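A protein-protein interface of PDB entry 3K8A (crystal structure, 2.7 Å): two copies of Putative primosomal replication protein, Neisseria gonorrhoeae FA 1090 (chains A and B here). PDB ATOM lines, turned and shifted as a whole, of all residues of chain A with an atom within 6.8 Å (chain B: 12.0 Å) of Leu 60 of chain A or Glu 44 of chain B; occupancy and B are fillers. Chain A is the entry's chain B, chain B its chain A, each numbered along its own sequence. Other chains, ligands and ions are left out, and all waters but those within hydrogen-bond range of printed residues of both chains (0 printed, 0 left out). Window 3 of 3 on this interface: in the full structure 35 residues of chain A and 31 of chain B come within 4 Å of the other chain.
The backbone carbonyl oxygen (O) of Glu 43 of chain B sits at hydrogen-bond distance from the side-chain amide nitrogen (NE2) of Gln 96 of chain A, at 3.3 Å.
The guanidinium group of Arg 58 of chain A lies within salt-bridge range of the side-chain carboxylate of Glu 44 of chain B (3.7 Å).
The side-chain carboxylate (OE2) of Glu 44 of chain B lies within salt-bridge range of the guanidinium group (NH1) of Arg 94 of chain A, 2.6 Å away.
N of Val 51 of chain B lies within hydrogen-bond range of O of Ser 40 of chain B (2.6 Å).
The backbone NH (N) of Cys 49 of chain B is in hydrogen-bond range of the backbone carbonyl oxygen (O) of Gln 42 of chain B, 2.8 Å away.
The side-chain amide nitrogen (NE2) of Gln 47 of chain B lies within hydrogen-bond range of the backbone carbonyl oxygen (O) of Glu 44 of chain B, at 2.9 Å.
N of Ile 95 of chain A is in hydrogen-bond range of O of Arg 58 of chain A (3.1 Å).
NE2 of Gln 63 of chain A sits at hydrogen-bond distance from O of Gln 96 of chain A (3.4 Å).
O of Phe 80 of chain A lies within hydrogen-bond range of N of Arg 94 of chain A, at 3.1 Å.
Among the printed residues, merely in contact across the chains: Leu 60 of chain A with Glu 44 of chain B (3.1 Å), Phe 80 of chain A with Gln 42 of chain B (3.8 Å), Phe 80 of chain A with Glu 43 of chain B (3.9 Å), Phe 80 of chain A with Val 51 of chain B (3.9 Å) and Gln 96 of chain A with Glu 44 of chain B (3.8 Å).
Leu 60 of chain A touches one residue of chain B.
Of chain A, only Arg 58 (3.7 Å), Leu 60 (3.1 Å), Arg 94 (2.6 Å) and Gln 96 (3.8 Å) come within 4 Å of Glu 44 of chain B.
No residue of chain B comes within 4 Å of Pro 30 of chain A.
No residue of chain B comes within 4 Å of Val 31 of chain A.
Of chain B, only Glu 44 (3.7 Å) comes within 4 Å of Arg 58 of chain A.
Ile 59 of chain A touches none of the printed residues of chain B.
No residue of chain B comes within 4 Å of Gly 61 of chain A.
No residue of chain B comes within 4 Å of Ala 64 of chain A.
Arg 94 of chain A touches just one residue of chain B: Glu 44 (2.6 Å).
Ile 95 of chain A touches none of the printed residues of chain B.
Gln 96 of chain A touches just these residues of chain B: Glu 43 and Glu 44.
Printed residues of chain A within 4 Å of Gln 42 of chain B: Phe 80 (3.8 Å).
Of the printed residues of chain A, Glu 43 of chain B touches Phe 80 and Gln 96.
Of the printed residues of chain A, Val 51 of chain B touches Phe 80.
Printed residues of chain B within 4 Å of Phe 80 of chain A: Gln 42, Glu 43 and Val 51.
The nearest printed residue of chain A that does not touch Gln 42 of chain B is Gln 96 of chain A (5.2 Å).
Printed residues of chain A that touch a printed residue of chain B: Arg 58, Leu 60, Phe 80, Arg 94 and Gln 96.
Hydrophobic or aromatic side chains of chain A that line the printed part of chain B: Leu 60 and Phe 80.
Along chain A the printed residues that touch a printed residue of chain B span positions 58 to 96.
Among the printed residues, Asp or Glu carboxylates within 4 Å of a Lys or Arg side-chain nitrogen of the other chain: Arg 58 of chain A with Glu 44 of chain B (3.7 Å) and Arg 94 of chain A with Glu 44 of chain B (2.6 Å).
No position is printed for both chains.
Of the 8 pairs that touch across the chains among the printed residues, none has its exchanged pair printed and touching as well.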
ATOM      1  N   THR A  25      -8.364 -13.565 -21.382  1.00  0.00           N
ATOM      2  CA  THR A  25      -7.822 -14.108 -20.145  1.00  0.00           C
ATOM      3  C   THR A  25      -8.702 -15.270 -19.790  1.00  0.00           C
ATOM      4  O   THR A  25      -9.770 -15.429 -20.378  1.00  0.00           O
ATOM      5  CB  THR A  25      -7.839 -13.091 -19.000  1.00  0.00           C
ATOM      6  OG1 THR A  25      -9.135 -13.072 -18.380  1.00  0.00           O
ATOM      7  CG2 THR A  25      -7.449 -11.678 -19.510  1.00  0.00           C
ATOM      8  N   ILE A  29     -12.098 -11.614 -19.968  1.00  0.00           N
ATOM      9  CA  ILE A  29     -11.603 -10.320 -20.442  1.00  0.00           C
ATOM     10  C   ILE A  29     -10.875 -10.359 -21.802  1.00  0.00           C
ATOM     11  O   ILE A  29      -9.961 -11.157 -22.006  1.00  0.00           O
ATOM     12  CB  ILE A  29     -10.673  -9.689 -19.394  1.00  0.00           C
ATOM     13  CG1 ILE A  29     -11.258  -9.881 -17.995  1.00  0.00           C
ATOM     14  CG2 ILE A  29     -10.435  -8.228 -19.698  1.00  0.00           C
ATOM     15  CD1 ILE A  29     -10.389  -9.328 -16.897  1.00  0.00           C
ATOM     16  N   PRO A  30     -11.276  -9.475 -22.731  1.00  0.00           N
ATOM     17  CA  PRO A  30     -10.702  -9.392 -24.079  1.00  0.00           C
ATOM     18  C   PRO A  30      -9.373  -8.635 -24.114  1.00  0.00           C
ATOM     19  O   PRO A  30      -9.275  -7.514 -23.605  1.00  0.00           O
ATOM     20  CB  PRO A  30     -11.764  -8.618 -24.877  1.00  0.00           C
ATOM     21  CG  PRO A  30     -12.948  -8.461 -23.951  1.00  0.00           C
ATOM     22  CD  PRO A  30     -12.406  -8.545 -22.565  1.00  0.00           C
ATOM     23  N   VAL A  31      -8.365  -9.265 -24.716  1.00  0.00           N
ATOM     24  CA  VAL A  31      -7.012  -8.729 -24.787  1.00  0.00           C
ATOM     25  C   VAL A  31      -6.621  -8.609 -26.253  1.00  0.00           C
ATOM     26  O   VAL A  31      -6.701  -9.581 -27.017  1.00  0.00           O
ATOM     27  CB  VAL A  31      -5.987  -9.634 -24.038  1.00  0.00           C
ATOM     28  CG1 VAL A  31      -4.599  -8.973 -23.990  1.00  0.00           C
ATOM     29  CG2 VAL A  31      -6.455  -9.921 -22.636  1.00  0.00           C
ATOM     30  N   LEU A  32      -6.219  -7.408 -26.640  1.00  0.00           N
ATOM     31  CA  LEU A  32      -5.790  -7.144 -27.998  1.00  0.00           C
ATOM     32  C   LEU A  32      -4.347  -6.650 -28.047  1.00  0.00           C
ATOM     33  O   LEU A  32      -4.063  -5.528 -27.628  1.00  0.00           O
ATOM     34  CB  LEU A  32      -6.681  -6.091 -28.632  1.00  0.00           C
ATOM     35  CG  LEU A  32      -6.195  -5.646 -30.009  1.00  0.00           C
ATOM     36  CD1 LEU A  32      -6.258  -6.811 -30.994  1.00  0.00           C
ATOM     37  CD2 LEU A  32      -6.998  -4.457 -30.504  1.00  0.00           C
ATOM     38  N   ARG A  58      -0.681  -2.960 -25.888  1.00  0.00           N
ATOM     39  CA  ARG A  58      -1.724  -3.855 -25.444  1.00  0.00           C
ATOM     40  C   ARG A  58      -2.949  -3.128 -24.868  1.00  0.00           C
ATOM     41  O   ARG A  58      -2.817  -2.294 -23.967  1.00  0.00           O
ATOM     42  CB  ARG A  58      -1.151  -4.788 -24.387  1.00  0.00           C
ATOM     43  CG  ARG A  58      -1.873  -6.086 -24.276  1.00  0.00           C
ATOM     44  CD  ARG A  58      -2.309  -6.278 -22.856  1.00  0.00           C
ATOM     45  NE  ARG A  58      -1.275  -6.802 -21.974  1.00  0.00           N
ATOM     46  CZ  ARG A  58      -1.304  -6.684 -20.646  1.00  0.00           C
ATOM     47  NH1 ARG A  58      -2.305  -6.040 -20.045  1.00  0.00           N
ATOM     48  NH2 ARG A  58      -0.321  -7.195 -19.910  1.00  0.00           N
ATOM     49  N   ILE A  59      -4.134  -3.465 -25.379  1.00  0.00           N
ATOM     50  CA  ILE A  59      -5.375  -2.902 -24.867  1.00  0.00           C
ATOM     51  C   ILE A  59      -6.195  -3.973 -24.163  1.00  0.00           C
ATOM     52  O   ILE A  59      -5.965  -5.156 -24.369  1.00  0.00           O
ATOM     53  CB  ILE A  59      -6.237  -2.306 -25.988  1.00  0.00           C
ATOM     54  CG1 ILE A  59      -5.351  -1.700 -27.077  1.00  0.00           C
ATOM     55  CG2 ILE A  59      -7.188  -1.267 -25.416  1.00  0.00           C
ATOM     56  CD1 ILE A  59      -6.121  -1.045 -28.201  1.00  0.00           C
ATOM     57  N   LEU A  60      -7.158  -3.554 -23.345  1.00  0.00           N
ATOM     58  CA  LEU A  60      -8.035  -4.500 -22.620  1.00  0.00           C
ATOM     59  C   LEU A  60      -9.515  -4.215 -22.799  1.00  0.00           C
ATOM     60  O   LEU A  60      -9.909  -3.175 -23.302  1.00  0.00           O
ATOM     61  CB  LEU A  60      -7.723  -4.525 -21.116  1.00  0.00           C
ATOM     62  CG  LEU A  60      -6.450  -5.232 -20.645  1.00  0.00           C
ATOM     63  CD1 LEU A  60      -6.358  -5.135 -19.125  1.00  0.00           C
ATOM     64  CD2 LEU A  60      -6.416  -6.691 -21.093  1.00  0.00           C
ATOM     65  N   GLY A  61     -10.330  -5.170 -22.372  1.00  0.00           N
ATOM     66  CA  GLY A  61     -11.780  -5.026 -22.338  1.00  0.00           C
ATOM     67  C   GLY A  61     -12.391  -4.281 -23.502  1.00  0.00           C
ATOM     68  O   GLY A  61     -12.120  -4.554 -24.667  1.00  0.00           O
ATOM     69  N   ARG A  62     -13.230  -3.322 -23.169  1.00  0.00           N
ATOM     70  CA  ARG A  62     -14.102  -2.700 -24.142  1.00  0.00           C
ATOM     71  C   ARG A  62     -13.428  -2.259 -25.455  1.00  0.00           C
ATOM     72  O   ARG A  62     -13.789  -2.736 -26.527  1.00  0.00           O
ATOM     73  CB  ARG A  62     -14.851  -1.553 -23.466  1.00  0.00           C
ATOM     74  CG  ARG A  62     -15.919  -0.983 -24.309  1.00  0.00           C
ATOM     75  CD  ARG A  62     -16.937  -0.264 -23.485  1.00  0.00           C
ATOM     76  NE  ARG A  62     -17.784   0.444 -24.421  1.00  0.00           N
ATOM     77  CZ  ARG A  62     -17.283   1.144 -25.431  1.00  0.00           C
ATOM     78  NH1 ARG A  62     -15.962   1.259 -25.543  1.00  0.00           N
ATOM     79  NH2 ARG A  62     -18.085   1.730 -26.313  1.00  0.00           N
ATOM     80  N   GLN A  63     -12.455  -1.348 -25.370  1.00  0.00           N
ATOM     81  CA  GLN A  63     -11.789  -0.818 -26.561  1.00  0.00           C
ATOM     82  C   GLN A  63     -10.995  -1.854 -27.354  1.00  0.00           C
ATOM     83  O   GLN A  63     -10.878  -1.748 -28.574  1.00  0.00           O
ATOM     84  CB  GLN A  63     -10.882   0.330 -26.174  1.00  0.00           C
ATOM     85  CG  GLN A  63     -11.627   1.475 -25.510  1.00  0.00           C
ATOM     86  CD  GLN A  63     -10.688   2.535 -24.982  1.00  0.00           C
ATOM     87  OE1 GLN A  63     -10.869   3.718 -25.252  1.00  0.00           O
ATOM     88  NE2 GLN A  63      -9.671   2.112 -24.227  1.00  0.00           N
ATOM     89  N   ALA A  64     -10.442  -2.848 -26.674  1.00  0.00           N
ATOM     90  CA  ALA A  64      -9.879  -4.001 -27.382  1.00  0.00           C
ATOM     91  C   ALA A  64     -10.868  -4.580 -28.406  1.00  0.00           C
ATOM     92  O   ALA A  64     -10.449  -5.152 -29.408  1.00  0.00           O
ATOM     93  CB  ALA A  64      -9.413  -5.076 -26.406  1.00  0.00           C
ATOM     94  N   GLU A  65     -12.172  -4.428 -28.157  1.00  0.00           N
ATOM     95  CA  GLU A  65     -13.212  -4.859 -29.101  1.00  0.00           C
ATOM     96  C   GLU A  65     -13.342  -3.967 -30.315  1.00  0.00           C
ATOM     97  O   GLU A  65     -13.392  -4.447 -31.447  1.00  0.00           O
ATOM     98  CB  GLU A  65     -14.590  -4.867 -28.435  1.00  0.00           C
ATOM     99  CG  GLU A  65     -15.185  -6.224 -28.249  1.00  0.00           C
ATOM    100  CD  GLU A  65     -14.251  -7.124 -27.495  1.00  0.00           C
ATOM    101  OE1 GLU A  65     -13.529  -6.582 -26.618  1.00  0.00           O
ATOM    102  OE2 GLU A  65     -14.222  -8.352 -27.792  1.00  0.00           O
ATOM    103  N   PHE A  80       0.701   3.905 -20.123  1.00  0.00           N
ATOM    104  CA  PHE A  80       1.946   3.910 -19.398  1.00  0.00           C
ATOM    105  C   PHE A  80       2.845   2.776 -19.866  1.00  0.00           C
ATOM    106  O   PHE A  80       2.370   1.755 -20.343  1.00  0.00           O
ATOM    107  CB  PHE A  80       1.675   3.803 -17.910  1.00  0.00           C
ATOM    108  CG  PHE A  80       0.828   2.638 -17.555  1.00  0.00           C
ATOM    109  CD1 PHE A  80      -0.536   2.788 -17.349  1.00  0.00           C
ATOM    110  CD2 PHE A  80       1.385   1.371 -17.453  1.00  0.00           C
ATOM    111  CE1 PHE A  80      -1.305   1.715 -17.042  1.00  0.00           C
ATOM    112  CE2 PHE A  80       0.614   0.285 -17.129  1.00  0.00           C
ATOM    113  CZ  PHE A  80      -0.728   0.450 -16.927  1.00  0.00           C
ATOM    114  N   ARG A  94       0.917  -0.004 -22.458  1.00  0.00           N
ATOM    115  CA  ARG A  94      -0.394  -0.490 -22.057  1.00  0.00           C
ATOM    116  C   ARG A  94      -1.398   0.649 -22.094  1.00  0.00           C
ATOM    117  O   ARG A  94      -1.437   1.516 -21.219  1.00  0.00           O
ATOM    118  CB  ARG A  94      -0.312  -1.138 -20.689  1.00  0.00           C
ATOM    119  CG  ARG A  94       0.937  -1.948 -20.603  1.00  0.00           C
ATOM    120  CD  ARG A  94       0.674  -3.376 -20.225  1.00  0.00           C
ATOM    121  NE  ARG A  94       0.989  -3.599 -18.831  1.00  0.00           N
ATOM    122  CZ  ARG A  94       0.072  -3.748 -17.893  1.00  0.00           C
ATOM    123  NH1 ARG A  94      -1.216  -3.726 -18.220  1.00  0.00           N
ATOM    124  NH2 ARG A  94       0.437  -3.945 -16.635  1.00  0.00           N
ATOM    125  N   ILE A  95      -2.197   0.620 -23.151  1.00  0.00           N
ATOM    126  CA  ILE A  95      -3.136   1.665 -23.511  1.00  0.00           C
ATOM    127  C   ILE A  95      -4.369   1.689 -22.622  1.00  0.00           C
ATOM    128  O   ILE A  95      -5.083   0.708 -22.548  1.00  0.00           O
ATOM    129  CB  ILE A  95      -3.576   1.459 -24.975  1.00  0.00           C
ATOM    130  CG1 ILE A  95      -2.340   1.381 -25.881  1.00  0.00           C
ATOM    131  CG2 ILE A  95      -4.560   2.541 -25.418  1.00  0.00           C
ATOM    132  CD1 ILE A  95      -2.581   0.755 -27.227  1.00  0.00           C
ATOM    133  N   GLN A  96      -4.592   2.823 -21.957  1.00  0.00           N
ATOM    134  CA  GLN A  96      -5.772   3.100 -21.146  1.00  0.00           C
ATOM    135  C   GLN A  96      -6.848   3.701 -22.004  1.00  0.00           C
ATOM    136  O   GLN A  96      -8.027   3.655 -21.666  1.00  0.00           O
ATOM    137  CB  GLN A  96      -5.457   4.185 -20.139  1.00  0.00           C
ATOM    138  CG  GLN A  96      -4.095   4.085 -19.537  1.00  0.00           C
ATOM    139  CD  GLN A  96      -4.137   3.244 -18.305  1.00  0.00           C
ATOM    140  OE1 GLN A  96      -4.604   2.093 -18.342  1.00  0.00           O
ATOM    141  NE2 GLN A  96      -3.675   3.812 -17.184  1.00  0.00           N
ATOM    142  N   SER B  40       6.097   1.573 -10.092  1.00  0.00           N
ATOM    143  CA  SER B  40       4.835   2.159  -9.597  1.00  0.00           C
ATOM    144  C   SER B  40       3.601   1.244  -9.606  1.00  0.00           C
ATOM    145  O   SER B  40       3.598   0.166 -10.201  1.00  0.00           O
ATOM    146  CB  SER B  40       4.489   3.410 -10.398  1.00  0.00           C
ATOM    147  OG  SER B  40       4.184   3.071 -11.750  1.00  0.00           O
ATOM    148  N   TRP B  41       2.547   1.709  -8.937  1.00  0.00           N
ATOM    149  CA  TRP B  41       1.208   1.115  -9.032  1.00  0.00           C
ATOM    150  C   TRP B  41       0.280   1.991  -9.906  1.00  0.00           C
ATOM    151  O   TRP B  41      -0.048   3.117  -9.538  1.00  0.00           O
ATOM    152  CB  TRP B  41       0.594   0.918  -7.640  1.00  0.00           C
ATOM    153  CG  TRP B  41       1.231  -0.179  -6.787  1.00  0.00           C
ATOM    154  CD1 TRP B  41       2.237  -0.024  -5.878  1.00  0.00           C
ATOM    155  CD2 TRP B  41       0.881  -1.579  -6.757  1.00  0.00           C
ATOM    156  NE1 TRP B  41       2.539  -1.230  -5.291  1.00  0.00           N
ATOM    157  CE2 TRP B  41       1.721  -2.199  -5.814  1.00  0.00           C
ATOM    158  CE3 TRP B  41      -0.051  -2.363  -7.443  1.00  0.00           C
ATOM    159  CZ2 TRP B  41       1.655  -3.568  -5.536  1.00  0.00           C
ATOM    160  CZ3 TRP B  41      -0.113  -3.718  -7.171  1.00  0.00           C
ATOM    161  CH2 TRP B  41       0.734  -4.305  -6.231  1.00  0.00           C
ATOM    162  N   GLN B  42      -0.117   1.473 -11.069  1.00  0.00           N
ATOM    163  CA  GLN B  42      -1.030   2.167 -11.968  1.00  0.00           C
ATOM    164  C   GLN B  42      -2.400   1.495 -11.978  1.00  0.00           C
ATOM    165  O   GLN B  42      -2.532   0.340 -11.586  1.00  0.00           O
ATOM    166  CB  GLN B  42      -0.468   2.198 -13.386  1.00  0.00           C
ATOM    167  CG  GLN B  42       0.935   2.801 -13.498  1.00  0.00           C
ATOM    168  CD  GLN B  42       0.974   4.246 -13.069  1.00  0.00           C
ATOM    169  OE1 GLN B  42       0.184   5.047 -13.547  1.00  0.00           O
ATOM    170  NE2 GLN B  42       1.884   4.585 -12.158  1.00  0.00           N
ATOM    171  N   GLU B  43      -3.412   2.246 -12.413  1.00  0.00           N
ATOM    172  CA  GLU B  43      -4.791   1.776 -12.513  1.00  0.00           C
ATOM    173  C   GLU B  43      -4.993   1.125 -13.880  1.00  0.00           C
ATOM    174  O   GLU B  43      -4.583   1.689 -14.892  1.00  0.00           O
ATOM    175  CB  GLU B  43      -5.758   2.958 -12.349  1.00  0.00           C
ATOM    176  CG  GLU B  43      -7.191   2.555 -12.087  1.00  0.00           C
ATOM    177  CD  GLU B  43      -7.341   1.860 -10.741  1.00  0.00           C
ATOM    178  OE1 GLU B  43      -6.418   2.006  -9.901  1.00  0.00           O
ATOM    179  OE2 GLU B  43      -8.363   1.169 -10.512  1.00  0.00           O
ATOM    180  N   GLU B  44      -5.580  -0.069 -13.924  1.00  0.00           N
ATOM    181  CA  GLU B  44      -5.906  -0.666 -15.220  1.00  0.00           C
ATOM    182  C   GLU B  44      -7.176  -1.474 -15.209  1.00  0.00           C
ATOM    183  O   GLU B  44      -7.281  -2.484 -14.531  1.00  0.00           O
ATOM    184  CB  GLU B  44      -4.764  -1.496 -15.819  1.00  0.00           C
ATOM    185  CG  GLU B  44      -4.862  -1.548 -17.362  1.00  0.00           C
ATOM    186  CD  GLU B  44      -3.941  -2.573 -18.059  1.00  0.00           C
ATOM    187  OE1 GLU B  44      -3.985  -3.777 -17.719  1.00  0.00           O
ATOM    188  OE2 GLU B  44      -3.208  -2.177 -18.993  1.00  0.00           O
ATOM    189  N   ASN B  45      -8.141  -1.023 -15.988  1.00  0.00           N
ATOM    190  CA  ASN B  45      -9.369  -1.754 -16.112  1.00  0.00           C
ATOM    191  C   ASN B  45      -9.896  -2.109 -14.728  1.00  0.00           C
ATOM    192  O   ASN B  45     -10.284  -3.240 -14.484  1.00  0.00           O
ATOM    193  CB  ASN B  45      -9.125  -3.016 -16.930  1.00  0.00           C
ATOM    194  CG  ASN B  45     -10.405  -3.705 -17.329  1.00  0.00           C
ATOM    195  OD1 ASN B  45     -11.313  -3.094 -17.898  1.00  0.00           O
ATOM    196  ND2 ASN B  45     -10.489  -4.991 -17.033  1.00  0.00           N
ATOM    197  N   GLY B  46      -9.879  -1.150 -13.810  1.00  0.00           N
ATOM    198  CA  GLY B  46     -10.488  -1.353 -12.507  1.00  0.00           C
ATOM    199  C   GLY B  46      -9.619  -1.778 -11.327  1.00  0.00           C
ATOM    200  O   GLY B  46     -10.043  -1.641 -10.183  1.00  0.00           O
ATOM    201  N   GLN B  47      -8.422  -2.318 -11.562  1.00  0.00           N
ATOM    202  CA  GLN B  47      -7.558  -2.660 -10.420  1.00  0.00           C
ATOM    203  C   GLN B  47      -6.167  -2.086 -10.512  1.00  0.00           C
ATOM    204  O   GLN B  47      -5.776  -1.555 -11.534  1.00  0.00           O
ATOM    205  CB  GLN B  47      -7.476  -4.156 -10.172  1.00  0.00           C
ATOM    206  CG  GLN B  47      -6.974  -4.927 -11.351  1.00  0.00           C
ATOM    207  CD  GLN B  47      -8.097  -5.319 -12.288  1.00  0.00           C
ATOM    208  OE1 GLN B  47      -9.178  -5.770 -11.851  1.00  0.00           O
ATOM    209  NE2 GLN B  47      -7.855  -5.154 -13.589  1.00  0.00           N
ATOM    210  N   GLN B  48      -5.422  -2.193  -9.425  1.00  0.00           N
ATOM    211  CA  GLN B  48      -4.110  -1.596  -9.363  1.00  0.00           C
ATOM    212  C   GLN B  48      -3.056  -2.610  -9.739  1.00  0.00           C
ATOM    213  O   GLN B  48      -3.236  -3.795  -9.517  1.00  0.00           O
ATOM    214  CB  GLN B  48      -3.861  -1.006  -7.983  1.00  0.00           C
ATOM    215  CG  GLN B  48      -4.963  -0.052  -7.558  1.00  0.00           C
ATOM    216  CD  GLN B  48      -4.464   1.027  -6.620  1.00  0.00           C
ATOM    217  OE1 GLN B  48      -3.425   1.640  -6.866  1.00  0.00           O
ATOM    218  NE2 GLN B  48      -5.204   1.265  -5.532  1.00  0.00           N
ATOM    219  N   CYS B  49      -1.957  -2.122 -10.307  1.00  0.00           N
ATOM    220  CA  CYS B  49      -0.950  -2.958 -10.956  1.00  0.00           C
ATOM    221  C   CYS B  49       0.462  -2.602 -10.599  1.00  0.00           C
ATOM    222  O   CYS B  49       0.864  -1.456 -10.731  1.00  0.00           O
ATOM    223  CB  CYS B  49      -1.050  -2.782 -12.457  1.00  0.00           C
ATOM    224  SG  CYS B  49      -2.476  -3.587 -13.016  1.00  0.00           S
ATOM    225  N   LEU B  50       1.233  -3.600 -10.198  1.00  0.00           N
ATOM    226  CA  LEU B  50       2.638  -3.372  -9.998  1.00  0.00           C
ATOM    227  C   LEU B  50       3.284  -3.204 -11.367  1.00  0.00           C
ATOM    228  O   LEU B  50       3.236  -4.113 -12.181  1.00  0.00           O
ATOM    229  CB  LEU B  50       3.272  -4.529  -9.231  1.00  0.00           C
ATOM    230  CG  LEU B  50       4.667  -4.173  -8.734  1.00  0.00           C
ATOM    231  CD1 LEU B  50       4.719  -2.690  -8.339  1.00  0.00           C
ATOM    232  CD2 LEU B  50       5.081  -5.061  -7.583  1.00  0.00           C
ATOM    233  N   VAL B  51       3.869  -2.037 -11.620  1.00  0.00           N
ATOM    234  CA  VAL B  51       4.569  -1.779 -12.873  1.00  0.00           C
ATOM    235  C   VAL B  51       6.089  -1.652 -12.673  1.00  0.00           C
ATOM    236  O   VAL B  51       6.536  -0.870 -11.847  1.00  0.00           O
ATOM    237  CB  VAL B  51       4.041  -0.494 -13.552  1.00  0.00           C
ATOM    238  CG1 VAL B  51       4.868  -0.165 -14.741  1.00  0.00           C
ATOM    239  CG2 VAL B  51       2.587  -0.665 -13.955  1.00  0.00           C
ATOM    240  N   GLN B  52       6.855  -2.428 -13.438  1.00  0.00           N
ATOM    241  CA  GLN B  52       8.309  -2.391 -13.446  1.00  0.00           C
ATOM    242  C   GLN B  52       8.773  -1.891 -14.800  1.00  0.00           C
ATOM    243  O   GLN B  52       8.240  -2.284 -15.819  1.00  0.00           O
ATOM    244  CB  GLN B  52       8.898  -3.786 -13.273  1.00  0.00           C
ATOM    245  CG  GLN B  52       8.646  -4.471 -11.938  1.00  0.00           C
ATOM    246  CD  GLN B  52       9.620  -5.636 -11.709  1.00  0.00           C
ATOM    247  OE1 GLN B  52      10.842  -5.440 -11.622  1.00  0.00           O
ATOM    248  NE2 GLN B  52       9.081  -6.850 -11.618  1.00  0.00           N
